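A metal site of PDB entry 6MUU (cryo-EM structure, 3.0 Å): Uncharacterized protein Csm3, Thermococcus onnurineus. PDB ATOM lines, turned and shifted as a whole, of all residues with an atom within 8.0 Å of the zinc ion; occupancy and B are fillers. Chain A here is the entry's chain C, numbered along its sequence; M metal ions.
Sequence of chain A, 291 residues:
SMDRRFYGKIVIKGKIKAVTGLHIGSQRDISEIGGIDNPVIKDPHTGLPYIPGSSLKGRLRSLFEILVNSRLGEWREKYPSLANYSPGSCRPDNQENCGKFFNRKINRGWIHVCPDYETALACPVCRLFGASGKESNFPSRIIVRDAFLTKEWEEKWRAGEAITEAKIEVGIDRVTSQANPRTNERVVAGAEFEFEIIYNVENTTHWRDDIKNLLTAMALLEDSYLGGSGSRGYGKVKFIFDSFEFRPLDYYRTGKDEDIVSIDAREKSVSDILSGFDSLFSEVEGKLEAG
A ring nitrogen (NE2) of His 112 binds the zinc ion, 1.8 Å away. The zinc ion is bound by the side-chain sulfur (SG) of Cys 123, at 2.0 Å. The zinc ion is bound by SG of Cys 114 (2.5 Å). SG of Cys 126 is bound to the zinc ion, 2.5 Å away. The zinc ion has four donor atoms within binding distance.
The side-chain sulfur (SG) of Cys 126 sits close to the guanidinium group (NH2) of Arg 61 (3.6 Å). The backbone carbonyl oxygen (O) of Phe 101 lies within hydrogen-bond range of a ring nitrogen (ND1) of His 112 (3.4 Å). SG of Cys 123 lies close to N of Val 125 (3.4 Å). The backbone carbonyl oxygen (O) of His 112 lies within hydrogen-bond range of the guanidinium group (NH2) of Arg 61, 3.3 Å away.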
ATOM      1  N   ARG A  61      17.585 -15.244 -21.974  1.00  0.00           N
ATOM      2  CA  ARG A  61      17.740 -14.492 -23.205  1.00  0.00           C
ATOM      3  C   ARG A  61      17.110 -15.228 -24.372  1.00  0.00           C
ATOM      4  O   ARG A  61      16.436 -14.620 -25.206  1.00  0.00           O
ATOM      5  CB  ARG A  61      19.218 -14.231 -23.491  1.00  0.00           C
ATOM      6  CG  ARG A  61      19.414 -13.254 -24.631  1.00  0.00           C
ATOM      7  CD  ARG A  61      20.848 -12.827 -24.802  1.00  0.00           C
ATOM      8  NE  ARG A  61      20.923 -11.781 -25.808  1.00  0.00           N
ATOM      9  CZ  ARG A  61      22.023 -11.102 -26.099  1.00  0.00           C
ATOM     10  NH1 ARG A  61      23.139 -11.364 -25.463  1.00  0.00           N
ATOM     11  NH2 ARG A  61      22.012 -10.156 -27.022  1.00  0.00           N
ATOM     12  N   GLU A  65      14.112 -13.730 -26.569  1.00  0.00           N
ATOM     13  CA  GLU A  65      14.289 -13.429 -27.985  1.00  0.00           C
ATOM     14  C   GLU A  65      13.204 -14.048 -28.844  1.00  0.00           C
ATOM     15  O   GLU A  65      12.839 -13.492 -29.878  1.00  0.00           O
ATOM     16  CB  GLU A  65      15.662 -13.889 -28.476  1.00  0.00           C
ATOM     17  CG  GLU A  65      16.816 -13.067 -27.990  1.00  0.00           C
ATOM     18  CD  GLU A  65      18.148 -13.575 -28.467  1.00  0.00           C
ATOM     19  OE1 GLU A  65      18.173 -14.587 -29.170  1.00  0.00           O
ATOM     20  OE2 GLU A  65      19.182 -12.993 -28.107  1.00  0.00           O
ATOM     21  N   VAL A  68      10.309 -11.698 -28.460  1.00  0.00           N
ATOM     22  CA  VAL A  68      10.455 -10.473 -29.252  1.00  0.00           C
ATOM     23  C   VAL A  68      10.357 -10.785 -30.736  1.00  0.00           C
ATOM     24  O   VAL A  68       9.855  -9.965 -31.513  1.00  0.00           O
ATOM     25  CB  VAL A  68      11.773  -9.780 -28.865  1.00  0.00           C
ATOM     26  CG1 VAL A  68      12.076  -8.573 -29.737  1.00  0.00           C
ATOM     27  CG2 VAL A  68      11.688  -9.322 -27.440  1.00  0.00           C
ATOM     28  N   SER A  81      14.473   0.333 -32.413  1.00  0.00           N
ATOM     29  CA  SER A  81      15.455  -0.483 -33.110  1.00  0.00           C
ATOM     30  C   SER A  81      14.882  -1.781 -33.666  1.00  0.00           C
ATOM     31  O   SER A  81      15.605  -2.532 -34.316  1.00  0.00           O
ATOM     32  CB  SER A  81      16.619  -0.808 -32.194  1.00  0.00           C
ATOM     33  OG  SER A  81      17.552  -1.633 -32.860  1.00  0.00           O
ATOM     34  N   LEU A  82      13.612  -2.065 -33.410  1.00  0.00           N
ATOM     35  CA  LEU A  82      12.979  -3.256 -33.942  1.00  0.00           C
ATOM     36  C   LEU A  82      12.307  -3.005 -35.276  1.00  0.00           C
ATOM     37  O   LEU A  82      11.663  -3.908 -35.813  1.00  0.00           O
ATOM     38  CB  LEU A  82      11.969  -3.825 -32.955  1.00  0.00           C
ATOM     39  CG  LEU A  82      12.530  -4.309 -31.613  1.00  0.00           C
ATOM     40  CD1 LEU A  82      11.396  -4.830 -30.765  1.00  0.00           C
ATOM     41  CD2 LEU A  82      13.588  -5.370 -31.832  1.00  0.00           C
ATOM     42  N   TYR A  85      14.217  -5.090 -38.284  1.00  0.00           N
ATOM     43  CA  TYR A  85      14.259  -6.535 -38.257  1.00  0.00           C
ATOM     44  C   TYR A  85      12.952  -7.128 -38.768  1.00  0.00           C
ATOM     45  O   TYR A  85      11.860  -6.659 -38.422  1.00  0.00           O
ATOM     46  CB  TYR A  85      14.550  -7.044 -36.848  1.00  0.00           C
ATOM     47  CG  TYR A  85      15.921  -6.665 -36.357  1.00  0.00           C
ATOM     48  CD1 TYR A  85      17.038  -7.331 -36.811  1.00  0.00           C
ATOM     49  CD2 TYR A  85      16.085  -5.636 -35.455  1.00  0.00           C
ATOM     50  CE1 TYR A  85      18.291  -6.997 -36.370  1.00  0.00           C
ATOM     51  CE2 TYR A  85      17.345  -5.294 -35.010  1.00  0.00           C
ATOM     52  CZ  TYR A  85      18.444  -5.981 -35.476  1.00  0.00           C
ATOM     53  OH  TYR A  85      19.696  -5.633 -35.034  1.00  0.00           O
ATOM     54  N   PHE A 101      15.893 -11.186 -37.774  1.00  0.00           N
ATOM     55  CA  PHE A 101      16.110 -10.911 -36.361  1.00  0.00           C
ATOM     56  C   PHE A 101      17.315 -11.674 -35.825  1.00  0.00           C
ATOM     57  O   PHE A 101      18.123 -11.105 -35.093  1.00  0.00           O
ATOM     58  CB  PHE A 101      14.849 -11.268 -35.560  1.00  0.00           C
ATOM     59  CG  PHE A 101      14.904 -10.839 -34.111  1.00  0.00           C
ATOM     60  CD1 PHE A 101      14.709  -9.508 -33.770  1.00  0.00           C
ATOM     61  CD2 PHE A 101      15.124 -11.760 -33.114  1.00  0.00           C
ATOM     62  CE1 PHE A 101      14.735  -9.118 -32.449  1.00  0.00           C
ATOM     63  CE2 PHE A 101      15.156 -11.363 -31.788  1.00  0.00           C
ATOM     64  CZ  PHE A 101      14.967 -10.044 -31.459  1.00  0.00           C
ATOM     65  N   ASN A 103      20.451 -12.415 -36.395  1.00  0.00           N
ATOM     66  CA  ASN A 103      21.416 -11.910 -37.362  1.00  0.00           C
ATOM     67  C   ASN A 103      22.857 -12.312 -37.074  1.00  0.00           C
ATOM     68  O   ASN A 103      23.598 -12.598 -38.013  1.00  0.00           O
ATOM     69  CB  ASN A 103      21.310 -10.384 -37.431  1.00  0.00           C
ATOM     70  CG  ASN A 103      21.431  -9.719 -36.071  1.00  0.00           C
ATOM     71  OD1 ASN A 103      21.650 -10.369 -35.066  1.00  0.00           O
ATOM     72  ND2 ASN A 103      21.290  -8.411 -36.053  1.00  0.00           N
ATOM     73  N   HIS A 112      20.241 -13.133 -32.131  1.00  0.00           N
ATOM     74  CA  HIS A 112      20.123 -11.673 -32.150  1.00  0.00           C
ATOM     75  C   HIS A 112      21.187 -11.052 -31.268  1.00  0.00           C
ATOM     76  O   HIS A 112      21.138 -11.205 -30.041  1.00  0.00           O
ATOM     77  CB  HIS A 112      18.753 -11.221 -31.694  1.00  0.00           C
ATOM     78  CG  HIS A 112      18.653  -9.740 -31.526  1.00  0.00           C
ATOM     79  ND1 HIS A 112      18.617  -8.879 -32.596  1.00  0.00           N
ATOM     80  CD2 HIS A 112      18.631  -8.967 -30.418  1.00  0.00           C
ATOM     81  CE1 HIS A 112      18.552  -7.634 -32.156  1.00  0.00           C
ATOM     82  NE2 HIS A 112      18.560  -7.661 -30.838  1.00  0.00           N
ATOM     83  N   VAL A 113      22.146 -10.349 -31.862  1.00  0.00           N
ATOM     84  CA  VAL A 113      23.015  -9.418 -31.162  1.00  0.00           C
ATOM     85  C   VAL A 113      23.081  -8.142 -31.999  1.00  0.00           C
ATOM     86  O   VAL A 113      23.423  -8.208 -33.192  1.00  0.00           O
ATOM     87  CB  VAL A 113      24.431  -9.973 -30.920  1.00  0.00           C
ATOM     88  CG1 VAL A 113      25.309  -8.920 -30.352  1.00  0.00           C
ATOM     89  CG2 VAL A 113      24.408 -11.143 -29.969  1.00  0.00           C
ATOM     90  N   CYS A 114      22.742  -7.009 -31.396  1.00  0.00           N
ATOM     91  CA  CYS A 114      22.763  -5.740 -32.120  1.00  0.00           C
ATOM     92  C   CYS A 114      24.194  -5.319 -32.433  1.00  0.00           C
ATOM     93  O   CYS A 114      25.113  -5.549 -31.643  1.00  0.00           O
ATOM     94  CB  CYS A 114      22.084  -4.648 -31.294  1.00  0.00           C
ATOM     95  SG  CYS A 114      20.298  -4.752 -31.237  1.00  0.00           S
ATOM     96  N   PRO A 115      24.421  -4.684 -33.579  1.00  0.00           N
ATOM     97  CA  PRO A 115      25.793  -4.405 -34.024  1.00  0.00           C
ATOM     98  C   PRO A 115      26.408  -3.091 -33.546  1.00  0.00           C
ATOM     99  O   PRO A 115      27.537  -2.793 -33.957  1.00  0.00           O
ATOM    100  CB  PRO A 115      25.647  -4.391 -35.547  1.00  0.00           C
ATOM    101  CG  PRO A 115      24.276  -3.915 -35.770  1.00  0.00           C
ATOM    102  CD  PRO A 115      23.453  -4.467 -34.666  1.00  0.00           C
ATOM    103  N   ASP A 116      25.741  -2.300 -32.717  1.00  0.00           N
ATOM    104  CA  ASP A 116      26.267  -0.987 -32.369  1.00  0.00           C
ATOM    105  C   ASP A 116      25.760  -0.619 -30.985  1.00  0.00           C
ATOM    106  O   ASP A 116      24.947  -1.325 -30.393  1.00  0.00           O
ATOM    107  CB  ASP A 116      25.853   0.039 -33.438  1.00  0.00           C
ATOM    108  CG  ASP A 116      26.720   1.284 -33.439  1.00  0.00           C
ATOM    109  OD1 ASP A 116      27.603   1.413 -32.572  1.00  0.00           O
ATOM    110  OD2 ASP A 116      26.513   2.143 -34.313  1.00  0.00           O
ATOM    111  N   THR A 119      22.099   1.255 -31.661  1.00  0.00           N
ATOM    112  CA  THR A 119      21.013   0.352 -31.976  1.00  0.00           C
ATOM    113  C   THR A 119      20.619  -0.498 -30.780  1.00  0.00           C
ATOM    114  O   THR A 119      19.429  -0.709 -30.535  1.00  0.00           O
ATOM    115  CB  THR A 119      21.386  -0.557 -33.140  1.00  0.00           C
ATOM    116  OG1 THR A 119      22.476  -1.396 -32.763  1.00  0.00           O
ATOM    117  CG2 THR A 119      21.800   0.286 -34.327  1.00  0.00           C
ATOM    118  N   ALA A 120      21.601  -0.972 -30.005  1.00  0.00           N
ATOM    119  CA  ALA A 120      21.318  -1.757 -28.804  1.00  0.00           C
ATOM    120  C   ALA A 120      20.763  -0.929 -27.664  1.00  0.00           C
ATOM    121  O   ALA A 120      20.289  -1.499 -26.685  1.00  0.00           O
ATOM    122  CB  ALA A 120      22.582  -2.469 -28.330  1.00  0.00           C
ATOM    123  N   LEU A 121      20.818   0.399 -27.767  1.00  0.00           N
ATOM    124  CA  LEU A 121      20.226   1.242 -26.736  1.00  0.00           C
ATOM    125  C   LEU A 121      18.708   1.223 -26.816  1.00  0.00           C
ATOM    126  O   LEU A 121      18.054   1.527 -25.814  1.00  0.00           O
ATOM    127  CB  LEU A 121      20.787   2.659 -26.880  1.00  0.00           C
ATOM    128  CG  LEU A 121      20.729   3.735 -25.789  1.00  0.00           C
ATOM    129  CD1 LEU A 121      19.411   4.488 -25.705  1.00  0.00           C
ATOM    130  CD2 LEU A 121      21.047   3.084 -24.463  1.00  0.00           C
ATOM    131  N   ALA A 122      18.130   0.846 -27.950  1.00  0.00           N
ATOM    132  CA  ALA A 122      16.689   0.866 -28.143  1.00  0.00           C
ATOM    133  C   ALA A 122      16.115  -0.480 -28.535  1.00  0.00           C
ATOM    134  O   ALA A 122      15.025  -0.543 -29.108  1.00  0.00           O
ATOM    135  CB  ALA A 122      16.316   1.926 -29.182  1.00  0.00           C
ATOM    136  N   CYS A 123      16.815  -1.570 -28.261  1.00  0.00           N
ATOM    137  CA  CYS A 123      16.383  -2.953 -28.398  1.00  0.00           C
ATOM    138  C   CYS A 123      15.965  -3.493 -27.047  1.00  0.00           C
ATOM    139  O   CYS A 123      16.672  -3.296 -26.065  1.00  0.00           O
ATOM    140  CB  CYS A 123      17.499  -3.815 -28.973  1.00  0.00           C
ATOM    141  SG  CYS A 123      17.131  -5.566 -29.070  1.00  0.00           S
ATOM    142  N   PRO A 124      14.823  -4.187 -26.944  1.00  0.00           N
ATOM    143  CA  PRO A 124      14.404  -4.713 -25.637  1.00  0.00           C
ATOM    144  C   PRO A 124      15.273  -5.859 -25.155  1.00  0.00           C
ATOM    145  O   PRO A 124      15.384  -6.062 -23.943  1.00  0.00           O
ATOM    146  CB  PRO A 124      12.973  -5.176 -25.900  1.00  0.00           C
ATOM    147  CG  PRO A 124      12.944  -5.491 -27.335  1.00  0.00           C
ATOM    148  CD  PRO A 124      13.844  -4.495 -27.993  1.00  0.00           C
ATOM    149  N   VAL A 125      15.872  -6.603 -26.080  1.00  0.00           N
ATOM    150  CA  VAL A 125      16.747  -7.709 -25.713  1.00  0.00           C
ATOM    151  C   VAL A 125      18.123  -7.204 -25.333  1.00  0.00           C
ATOM    152  O   VAL A 125      18.688  -7.619 -24.323  1.00  0.00           O
ATOM    153  CB  VAL A 125      16.807  -8.707 -26.881  1.00  0.00           C
ATOM    154  CG1 VAL A 125      17.807  -9.804 -26.595  1.00  0.00           C
ATOM    155  CG2 VAL A 125      15.452  -9.294 -27.139  1.00  0.00           C
ATOM    156  N   CYS A 126      18.680  -6.293 -26.116  1.00  0.00           N
ATOM    157  CA  CYS A 126      20.082  -5.932 -25.994  1.00  0.00           C
ATOM    158  C   CYS A 126      20.332  -4.746 -25.082  1.00  0.00           C
ATOM    159  O   CYS A 126      21.490  -4.557 -24.677  1.00  0.00           O
ATOM    160  CB  CYS A 126      20.675  -5.642 -27.359  1.00  0.00           C
ATOM    161  SG  CYS A 126      20.719  -7.056 -28.447  1.00  0.00           S
ATOM    162  N   ARG A 127      19.320  -3.941 -24.729  1.00  0.00           N
ATOM    163  CA  ARG A 127      19.563  -2.958 -23.676  1.00  0.00           C
ATOM    164  C   ARG A 127      19.683  -3.635 -22.326  1.00  0.00           C
ATOM    165  O   ARG A 127      20.265  -3.051 -21.402  1.00  0.00           O
ATOM    166  CB  ARG A 127      18.472  -1.890 -23.602  1.00  0.00           C
ATOM    167  CG  ARG A 127      17.178  -2.370 -22.994  1.00  0.00           C
ATOM    168  CD  ARG A 127      16.196  -1.267 -22.690  1.00  0.00           C
ATOM    169  NE  ARG A 127      15.628  -0.638 -23.867  1.00  0.00           N
ATOM    170  CZ  ARG A 127      14.785   0.379 -23.806  1.00  0.00           C
ATOM    171  NH1 ARG A 127      14.401   0.855 -22.633  1.00  0.00           N
ATOM    172  NH2 ARG A 127      14.300   0.920 -24.932  1.00  0.00           N
ATOM    173  N   LEU A 128      19.167  -4.855 -22.186  1.00  0.00           N
ATOM    174  CA  LEU A 128      19.164  -5.602 -20.952  1.00  0.00           C
ATOM    175  C   LEU A 128      20.254  -6.646 -20.906  1.00  0.00           C
ATOM    176  O   LEU A 128      21.010  -6.717 -19.930  1.00  0.00           O
ATOM    177  CB  LEU A 128      17.799  -6.260 -20.779  1.00  0.00           C
ATOM    178  CG  LEU A 128      17.551  -6.956 -19.448  1.00  0.00           C
ATOM    179  CD1 LEU A 128      17.556  -5.914 -18.386  1.00  0.00           C
ATOM    180  CD2 LEU A 128      16.239  -7.671 -19.477  1.00  0.00           C
ATOM    181  N   GLY A 130      22.736  -7.129 -23.378  1.00  0.00           N
ATOM    182  CA  GLY A 130      23.995  -6.667 -23.893  1.00  0.00           C
ATOM    183  C   GLY A 130      24.223  -7.053 -25.341  1.00  0.00           C
ATOM    184  O   GLY A 130      23.550  -7.920 -25.898  1.00  0.00           O
ATOM    185  N   ALA A 131      25.188  -6.396 -25.964  1.00  0.00           N
ATOM    186  CA  ALA A 131      25.520  -6.633 -27.348  1.00  0.00           C
ATOM    187  C   ALA A 131      27.029  -6.522 -27.532  1.00  0.00           C
ATOM    188  O   ALA A 131      27.681  -5.706 -26.893  1.00  0.00           O
ATOM    189  CB  ALA A 131      24.821  -5.638 -28.278  1.00  0.00           C
HETATM  190 ZN    ZN M   1      18.809  -6.194 -29.845  1.00  0.00          ZN
